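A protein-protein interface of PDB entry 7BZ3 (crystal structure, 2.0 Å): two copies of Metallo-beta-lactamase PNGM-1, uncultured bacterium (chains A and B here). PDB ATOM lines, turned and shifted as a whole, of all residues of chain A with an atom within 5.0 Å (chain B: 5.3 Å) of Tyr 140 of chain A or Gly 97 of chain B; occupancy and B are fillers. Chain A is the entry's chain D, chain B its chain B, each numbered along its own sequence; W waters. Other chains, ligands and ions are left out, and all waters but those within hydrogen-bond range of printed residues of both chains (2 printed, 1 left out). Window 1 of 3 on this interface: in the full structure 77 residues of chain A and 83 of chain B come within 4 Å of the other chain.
The backbone NH (N) of Thr 93 of chain B lies within hydrogen-bond range of the side-chain carboxylate (OD2) of Asp 143 of chain A (3.4 Å).
Among the printed residues, merely in contact across the chains: Tyr 140 of chain A with Trp 96 of chain B (3.3 Å), Val 100 of chain A with Thr 93 of chain B (3.5 Å), Asp 143 of chain A with His 92 of chain B (3.5 Å), Trp 142 of chain A with His 92 of chain B (3.6 Å), Ala 139 of chain A with Trp 96 of chain B (3.7 Å), Tyr 140 of chain A with Thr 93 of chain B (3.7 Å), Tyr 140 of chain A with Gly 97 of chain B (3.8 Å), Trp 142 of chain A with Leu 91 of chain B (3.9 Å) and Asp 143 of chain A with Leu 91 of chain B (3.95 Å).
Water W2 lies within hydrogen-bond range of O of Leu 91 of chain B (2.7 Å), N of Asp 143 of chain A (2.9 Å) and O of Tyr 140 of chain A (3.3 Å).
Water W1 lies within hydrogen-bond range of O of Trp 96 of chain B (3.1 Å), N of Val 100 of chain B (3.2 Å), OH of Tyr 140 of chain A (3.4 Å) and O of Gly 97 of chain B (3.5 Å).
1 position is printed for both chains.
Of the 10 pairs that touch across the chains among the printed residues, none has its exchanged pair printed and touching as well.
Printed residues of chain B within 4 Å of Val 100 of chain A: Thr 93.
Of the printed residues of chain B, Tyr 140 of chain A touches Thr 93, Trp 96 and Gly 97.
Of the printed residues of chain A, His 92 of chain B touches Trp 142 and Asp 143.
Of the printed residues of chain A, Gly 97 of chain B touches Tyr 140.
Asp 98 of chain B touches none of the printed residues of chain A.
Leu 99 of chain B touches none of the printed residues of chain A.
The nearest printed residue of chain B that does not touch Tyr 140 of chain A is Leu 91 of chain B (4.02 Å).
Printed residues of chain B that touch a printed residue of chain A: Leu 91, His 92, Thr 93, Trp 96 and Gly 97.
Hydrophobic or aromatic side chains of chain B that line the printed part of chain A: Leu 91, His 92 and Trp 96.
Of the 11 printed residues of chain A, 5 touch a printed residue of chain B.
Along chain A the printed residues that touch a printed residue of chain B span positions 100 to 143.
Among the printed residues, 10 pairs touch across the chains.
Among the printed residues, no Asp or Glu carboxylate lies within 4 Å of a Lys or Arg side-chain nitrogen of the other chain.
The backbone carbonyl oxygen of Leu 91 of chain B lies within hydrogen-bond range of the indole nitrogen of Trp 96 of chain B, at 3.0 Å.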
ATOM      1  N   VAL A 100      22.744  30.526  12.644  1.00  0.00           N
ATOM      2  CA  VAL A 100      24.006  29.736  12.743  1.00  0.00           C
ATOM      3  C   VAL A 100      25.208  30.686  12.706  1.00  0.00           C
ATOM      4  O   VAL A 100      26.148  30.472  13.488  1.00  0.00           O
ATOM      5  CB  VAL A 100      24.096  28.636  11.663  1.00  0.00           C
ATOM      6  CG1 VAL A 100      24.288  29.183  10.253  1.00  0.00           C
ATOM      7  CG2 VAL A 100      25.204  27.644  12.000  1.00  0.00           C
ATOM      8  N   TRP A 103      25.365  32.256  15.993  1.00  0.00           N
ATOM      9  CA  TRP A 103      25.804  31.181  16.914  1.00  0.00           C
ATOM     10  C   TRP A 103      27.332  30.983  16.824  1.00  0.00           C
ATOM     11  O   TRP A 103      27.986  31.053  17.867  1.00  0.00           O
ATOM     12  CB  TRP A 103      25.020  29.897  16.621  1.00  0.00           C
ATOM     13  CG  TRP A 103      25.539  28.698  17.344  1.00  0.00           C
ATOM     14  CD1 TRP A 103      25.422  28.438  18.669  1.00  0.00           C
ATOM     15  CD2 TRP A 103      26.233  27.580  16.772  1.00  0.00           C
ATOM     16  NE1 TRP A 103      26.042  27.262  18.966  1.00  0.00           N
ATOM     17  CE2 TRP A 103      26.546  26.710  17.825  1.00  0.00           C
ATOM     18  CE3 TRP A 103      26.650  27.243  15.488  1.00  0.00           C
ATOM     19  CZ2 TRP A 103      27.227  25.511  17.635  1.00  0.00           C
ATOM     20  CZ3 TRP A 103      27.332  26.064  15.297  1.00  0.00           C
ATOM     21  CH2 TRP A 103      27.642  25.222  16.361  1.00  0.00           C
ATOM     22  N   MET A 136      19.222  22.235  14.241  1.00  0.00           N
ATOM     23  CA  MET A 136      20.183  23.212  13.677  1.00  0.00           C
ATOM     24  C   MET A 136      21.553  22.967  14.311  1.00  0.00           C
ATOM     25  O   MET A 136      22.555  22.928  13.576  1.00  0.00           O
ATOM     26  CB  MET A 136      19.742  24.662  13.893  1.00  0.00           C
ATOM     27  CG  MET A 136      20.606  25.653  13.113  1.00  0.00           C
ATOM     28  SD  MET A 136      21.019  27.218  13.994  1.00  0.00           S
ATOM     29  CE  MET A 136      21.978  26.577  15.362  1.00  0.00           C
ATOM     30  N   LEU A 137      21.595  22.904  15.637  1.00  0.00           N
ATOM     31  CA  LEU A 137      22.821  22.588  16.399  1.00  0.00           C
ATOM     32  C   LEU A 137      23.315  21.186  16.071  1.00  0.00           C
ATOM     33  O   LEU A 137      24.518  21.056  16.020  1.00  0.00           O
ATOM     34  CB  LEU A 137      22.543  22.728  17.896  1.00  0.00           C
ATOM     35  CG  LEU A 137      22.213  24.158  18.337  1.00  0.00           C
ATOM     36  CD1 LEU A 137      21.840  24.174  19.806  1.00  0.00           C
ATOM     37  CD2 LEU A 137      23.355  25.106  18.072  1.00  0.00           C
ATOM     38  N   LYS A 138      22.462  20.160  15.908  1.00  0.00           N
ATOM     39  CA  LYS A 138      22.982  18.827  15.456  1.00  0.00           C
ATOM     40  C   LYS A 138      23.565  18.926  14.031  1.00  0.00           C
ATOM     41  O   LYS A 138      24.606  18.226  13.726  1.00  0.00           O
ATOM     42  CB  LYS A 138      21.898  17.756  15.535  1.00  0.00           C
ATOM     43  CG  LYS A 138      21.488  17.337  16.932  1.00  0.00           C
ATOM     44  CD  LYS A 138      20.406  16.267  16.961  1.00  0.00           C
ATOM     45  CE  LYS A 138      19.723  16.125  18.316  1.00  0.00           C
ATOM     46  NZ  LYS A 138      20.627  15.603  19.363  1.00  0.00           N
ATOM     47  N   ALA A 139      22.975  19.768  13.166  1.00  0.00           N
ATOM     48  CA  ALA A 139      23.500  19.986  11.804  1.00  0.00           C
ATOM     49  C   ALA A 139      24.985  20.351  11.871  1.00  0.00           C
ATOM     50  O   ALA A 139      25.747  19.865  10.999  1.00  0.00           O
ATOM     51  CB  ALA A 139      22.704  21.034  11.069  1.00  0.00           C
ATOM     52  N   TYR A 140      25.395  21.179  12.855  1.00  0.00           N
ATOM     53  CA  TYR A 140      26.758  21.756  12.909  1.00  0.00           C
ATOM     54  C   TYR A 140      27.518  21.114  14.070  1.00  0.00           C
ATOM     55  O   TYR A 140      28.323  21.801  14.660  1.00  0.00           O
ATOM     56  CB  TYR A 140      26.724  23.296  12.992  1.00  0.00           C
ATOM     57  CG  TYR A 140      26.211  23.984  11.751  1.00  0.00           C
ATOM     58  CD1 TYR A 140      24.847  24.161  11.549  1.00  0.00           C
ATOM     59  CD2 TYR A 140      27.074  24.467  10.776  1.00  0.00           C
ATOM     60  CE1 TYR A 140      24.355  24.766  10.406  1.00  0.00           C
ATOM     61  CE2 TYR A 140      26.595  25.084   9.633  1.00  0.00           C
ATOM     62  CZ  TYR A 140      25.234  25.236   9.444  1.00  0.00           C
ATOM     63  OH  TYR A 140      24.731  25.825   8.309  1.00  0.00           O
ATOM     64  N   ASN A 141      27.288  19.827  14.349  1.00  0.00           N
ATOM     65  CA  ASN A 141      28.025  19.054  15.379  1.00  0.00           C
ATOM     66  C   ASN A 141      29.536  19.093  15.105  1.00  0.00           C
ATOM     67  O   ASN A 141      30.279  19.234  16.059  1.00  0.00           O
ATOM     68  CB  ASN A 141      27.535  17.600  15.436  1.00  0.00           C
ATOM     69  CG  ASN A 141      28.093  16.858  16.630  1.00  0.00           C
ATOM     70  OD1 ASN A 141      27.904  17.301  17.753  1.00  0.00           O
ATOM     71  ND2 ASN A 141      28.832  15.780  16.382  1.00  0.00           N
ATOM     72  N   TRP A 142      29.998  18.875  13.865  1.00  0.00           N
ATOM     73  CA  TRP A 142      31.461  18.842  13.566  1.00  0.00           C
ATOM     74  C   TRP A 142      32.114  20.192  13.945  1.00  0.00           C
ATOM     75  O   TRP A 142      33.129  20.167  14.661  1.00  0.00           O
ATOM     76  CB  TRP A 142      31.709  18.461  12.102  1.00  0.00           C
ATOM     77  CG  TRP A 142      33.163  18.419  11.795  1.00  0.00           C
ATOM     78  CD1 TRP A 142      33.948  17.309  11.809  1.00  0.00           C
ATOM     79  CD2 TRP A 142      34.024  19.520  11.452  1.00  0.00           C
ATOM     80  NE1 TRP A 142      35.230  17.638  11.482  1.00  0.00           N
ATOM     81  CE2 TRP A 142      35.311  18.988  11.259  1.00  0.00           C
ATOM     82  CE3 TRP A 142      33.842  20.888  11.240  1.00  0.00           C
ATOM     83  CZ2 TRP A 142      36.404  19.780  10.912  1.00  0.00           C
ATOM     84  CZ3 TRP A 142      34.920  21.673  10.878  1.00  0.00           C
ATOM     85  CH2 TRP A 142      36.185  21.122  10.724  1.00  0.00           C
ATOM     86  N   ASP A 143      31.563  21.329  13.499  1.00  0.00           N
ATOM     87  CA  ASP A 143      31.921  22.697  14.015  1.00  0.00           C
ATOM     88  C   ASP A 143      31.947  22.655  15.557  1.00  0.00           C
ATOM     89  O   ASP A 143      33.017  22.941  16.179  1.00  0.00           O
ATOM     90  CB  ASP A 143      30.930  23.745  13.475  1.00  0.00           C
ATOM     91  CG  ASP A 143      31.334  25.219  13.457  1.00  0.00           C
ATOM     92  OD1 ASP A 143      32.016  25.653  14.357  1.00  0.00           O
ATOM     93  OD2 ASP A 143      30.977  25.923  12.486  1.00  0.00           O
ATOM     94  N   TYR A 144      30.821  22.290  16.175  1.00  0.00           N
ATOM     95  CA  TYR A 144      30.662  22.335  17.655  1.00  0.00           C
ATOM     96  C   TYR A 144      31.776  21.512  18.306  1.00  0.00           C
ATOM     97  O   TYR A 144      32.570  22.042  19.138  1.00  0.00           O
ATOM     98  CB  TYR A 144      29.300  21.809  18.129  1.00  0.00           C
ATOM     99  CG  TYR A 144      29.175  21.749  19.637  1.00  0.00           C
ATOM    100  CD1 TYR A 144      29.005  22.910  20.389  1.00  0.00           C
ATOM    101  CD2 TYR A 144      29.297  20.550  20.322  1.00  0.00           C
ATOM    102  CE1 TYR A 144      28.911  22.877  21.773  1.00  0.00           C
ATOM    103  CE2 TYR A 144      29.231  20.505  21.712  1.00  0.00           C
ATOM    104  CZ  TYR A 144      29.040  21.668  22.439  1.00  0.00           C
ATOM    105  OH  TYR A 144      28.915  21.594  23.793  1.00  0.00           O
ATOM    106  N   ILE B  65      29.985  26.961  -0.017  1.00  0.00           N
ATOM    107  CA  ILE B  65      28.878  27.934  -0.174  1.00  0.00           C
ATOM    108  C   ILE B  65      28.639  28.580   1.194  1.00  0.00           C
ATOM    109  O   ILE B  65      27.543  28.352   1.847  1.00  0.00           O
ATOM    110  CB  ILE B  65      27.679  27.248  -0.861  1.00  0.00           C
ATOM    111  CG1 ILE B  65      26.563  28.248  -1.191  1.00  0.00           C
ATOM    112  CG2 ILE B  65      27.169  26.043  -0.062  1.00  0.00           C
ATOM    113  CD1 ILE B  65      25.530  27.683  -2.119  1.00  0.00           C
ATOM    114  N   GLY B  66      29.641  29.376   1.608  1.00  0.00           N
ATOM    115  CA  GLY B  66      29.720  30.044   2.914  1.00  0.00           C
ATOM    116  C   GLY B  66      28.566  31.015   3.112  1.00  0.00           C
ATOM    117  O   GLY B  66      27.997  31.491   2.086  1.00  0.00           O
ATOM    118  N   SER B  67      28.194  31.228   4.374  1.00  0.00           N
ATOM    119  CA  SER B  67      27.269  32.298   4.846  1.00  0.00           C
ATOM    120  C   SER B  67      27.511  33.546   4.010  1.00  0.00           C
ATOM    121  O   SER B  67      28.683  34.000   3.861  1.00  0.00           O
ATOM    122  CB  SER B  67      27.426  32.604   6.332  1.00  0.00           C
ATOM    123  OG  SER B  67      27.100  31.470   7.155  1.00  0.00           O
ATOM    124  N   LEU B  91      32.850  21.355   7.246  1.00  0.00           N
ATOM    125  CA  LEU B  91      31.500  21.629   7.817  1.00  0.00           C
ATOM    126  C   LEU B  91      31.520  22.860   8.742  1.00  0.00           C
ATOM    127  O   LEU B  91      30.607  22.948   9.618  1.00  0.00           O
ATOM    128  CB  LEU B  91      30.986  20.370   8.535  1.00  0.00           C
ATOM    129  CG  LEU B  91      30.867  19.129   7.627  1.00  0.00           C
ATOM    130  CD1 LEU B  91      30.657  17.872   8.434  1.00  0.00           C
ATOM    131  CD2 LEU B  91      29.776  19.274   6.579  1.00  0.00           C
ATOM    132  N   HIS B  92      32.449  23.809   8.521  1.00  0.00           N
ATOM    133  CA  HIS B  92      32.396  25.165   9.134  1.00  0.00           C
ATOM    134  C   HIS B  92      31.341  26.015   8.438  1.00  0.00           C
ATOM    135  O   HIS B  92      31.270  25.954   7.166  1.00  0.00           O
ATOM    136  CB  HIS B  92      33.740  25.897   9.105  1.00  0.00           C
ATOM    137  CG  HIS B  92      34.603  25.541  10.260  1.00  0.00           C
ATOM    138  ND1 HIS B  92      35.945  25.411  10.127  1.00  0.00           N
ATOM    139  CD2 HIS B  92      34.301  25.324  11.563  1.00  0.00           C
ATOM    140  CE1 HIS B  92      36.462  25.065  11.284  1.00  0.00           C
ATOM    141  NE2 HIS B  92      35.479  25.027  12.195  1.00  0.00           N
ATOM    142  N   THR B  93      30.581  26.774   9.245  1.00  0.00           N
ATOM    143  CA  THR B  93      29.572  27.774   8.790  1.00  0.00           C
ATOM    144  C   THR B  93      30.139  28.583   7.598  1.00  0.00           C
ATOM    145  O   THR B  93      29.465  28.741   6.598  1.00  0.00           O
ATOM    146  CB  THR B  93      29.130  28.672   9.951  1.00  0.00           C
ATOM    147  OG1 THR B  93      30.290  29.403  10.344  1.00  0.00           O
ATOM    148  CG2 THR B  93      28.540  27.915  11.124  1.00  0.00           C
ATOM    149  N   ASP B  94      31.392  29.017   7.658  1.00  0.00           N
ATOM    150  CA  ASP B  94      31.962  29.853   6.582  1.00  0.00           C
ATOM    151  C   ASP B  94      32.235  29.030   5.310  1.00  0.00           C
ATOM    152  O   ASP B  94      32.756  29.633   4.402  1.00  0.00           O
ATOM    153  CB  ASP B  94      33.163  30.655   7.075  1.00  0.00           C
ATOM    154  CG  ASP B  94      34.356  29.824   7.521  1.00  0.00           C
ATOM    155  OD1 ASP B  94      34.199  29.066   8.463  1.00  0.00           O
ATOM    156  OD2 ASP B  94      35.413  29.965   6.936  1.00  0.00           O
ATOM    157  N   HIS B  95      31.855  27.732   5.213  1.00  0.00           N
ATOM    158  CA  HIS B  95      31.998  26.926   3.966  1.00  0.00           C
ATOM    159  C   HIS B  95      30.707  26.223   3.530  1.00  0.00           C
ATOM    160  O   HIS B  95      30.764  25.628   2.432  1.00  0.00           O
ATOM    161  CB  HIS B  95      33.146  25.915   4.083  1.00  0.00           C
ATOM    162  CG  HIS B  95      34.457  26.589   4.294  1.00  0.00           C
ATOM    163  ND1 HIS B  95      35.361  26.801   3.256  1.00  0.00           N
ATOM    164  CD2 HIS B  95      34.959  27.221   5.373  1.00  0.00           C
ATOM    165  CE1 HIS B  95      36.382  27.461   3.716  1.00  0.00           C
ATOM    166  NE2 HIS B  95      36.173  27.710   5.007  1.00  0.00           N
ATOM    167  N   TRP B  96      29.628  26.244   4.327  1.00  0.00           N
ATOM    168  CA  TRP B  96      28.327  25.654   3.925  1.00  0.00           C
ATOM    169  C   TRP B  96      27.108  26.326   4.583  1.00  0.00           C
ATOM    170  O   TRP B  96      25.998  25.801   4.372  1.00  0.00           O
ATOM    171  CB  TRP B  96      28.342  24.134   4.088  1.00  0.00           C
ATOM    172  CG  TRP B  96      28.074  23.605   5.454  1.00  0.00           C
ATOM    173  CD1 TRP B  96      28.883  23.701   6.549  1.00  0.00           C
ATOM    174  CD2 TRP B  96      26.914  22.876   5.873  1.00  0.00           C
ATOM    175  NE1 TRP B  96      28.315  23.077   7.611  1.00  0.00           N
ATOM    176  CE2 TRP B  96      27.097  22.579   7.232  1.00  0.00           C
ATOM    177  CE3 TRP B  96      25.761  22.414   5.219  1.00  0.00           C
ATOM    178  CZ2 TRP B  96      26.167  21.849   7.963  1.00  0.00           C
ATOM    179  CZ3 TRP B  96      24.833  21.722   5.954  1.00  0.00           C
ATOM    180  CH2 TRP B  96      25.032  21.453   7.309  1.00  0.00           C
ATOM    181  N   GLY B  97      27.277  27.480   5.246  1.00  0.00           N
ATOM    182  CA  GLY B  97      26.166  28.260   5.831  1.00  0.00           C
ATOM    183  C   GLY B  97      25.067  28.543   4.825  1.00  0.00           C
ATOM    184  O   GLY B  97      23.934  28.578   5.209  1.00  0.00           O
ATOM    185  N   ASP B  98      25.388  28.793   3.558  1.00  0.00           N
ATOM    186  CA  ASP B  98      24.359  29.234   2.592  1.00  0.00           C
ATOM    187  C   ASP B  98      23.838  28.004   1.852  1.00  0.00           C
ATOM    188  O   ASP B  98      23.110  28.212   0.872  1.00  0.00           O
ATOM    189  CB  ASP B  98      24.831  30.375   1.666  1.00  0.00           C
ATOM    190  CG  ASP B  98      24.456  31.780   2.154  1.00  0.00           C
ATOM    191  OD1 ASP B  98      24.042  31.895   3.387  1.00  0.00           O
ATOM    192  OD2 ASP B  98      24.674  32.778   1.361  1.00  0.00           O
ATOM    193  N   LEU B  99      24.172  26.762   2.247  1.00  0.00           N
ATOM    194  CA  LEU B  99      23.550  25.595   1.558  1.00  0.00           C
ATOM    195  C   LEU B  99      22.026  25.734   1.639  1.00  0.00           C
ATOM    196  O   LEU B  99      21.372  25.669   0.590  1.00  0.00           O
ATOM    197  CB  LEU B  99      23.953  24.250   2.154  1.00  0.00           C
ATOM    198  CG  LEU B  99      23.397  23.040   1.392  1.00  0.00           C
ATOM    199  CD1 LEU B  99      23.880  23.044  -0.038  1.00  0.00           C
ATOM    200  CD2 LEU B  99      23.773  21.746   2.081  1.00  0.00           C
ATOM    201  N   VAL B 100      21.501  25.983   2.840  1.00  0.00           N
ATOM    202  CA  VAL B 100      20.030  26.098   3.078  1.00  0.00           C
ATOM    203  C   VAL B 100      19.431  27.161   2.156  1.00  0.00           C
ATOM    204  O   VAL B 100      18.299  26.966   1.761  1.00  0.00           O
ATOM    205  CB  VAL B 100      19.693  26.375   4.554  1.00  0.00           C
ATOM    206  CG1 VAL B 100      20.285  27.665   5.070  1.00  0.00           C
ATOM    207  CG2 VAL B 100      18.185  26.380   4.790  1.00  0.00           C
ATOM    208  N   SER B 101      20.152  28.252   1.824  1.00  0.00           N
ATOM    209  CA  SER B 101      19.610  29.326   0.942  1.00  0.00           C
ATOM    210  C   SER B 101      19.671  28.851  -0.512  1.00  0.00           C
ATOM    211  O   SER B 101      18.719  29.092  -1.299  1.00  0.00           O
ATOM    212  CB  SER B 101      20.304  30.645   1.139  1.00  0.00           C
ATOM    213  OG  SER B 101      19.672  31.649   0.364  1.00  0.00           O
HETATM  214  O   HOH W   1      23.152  25.181   5.425  1.00  0.00           O
HETATM  215  O   HOH W   2      29.483  21.502  11.540  1.00  0.00           O
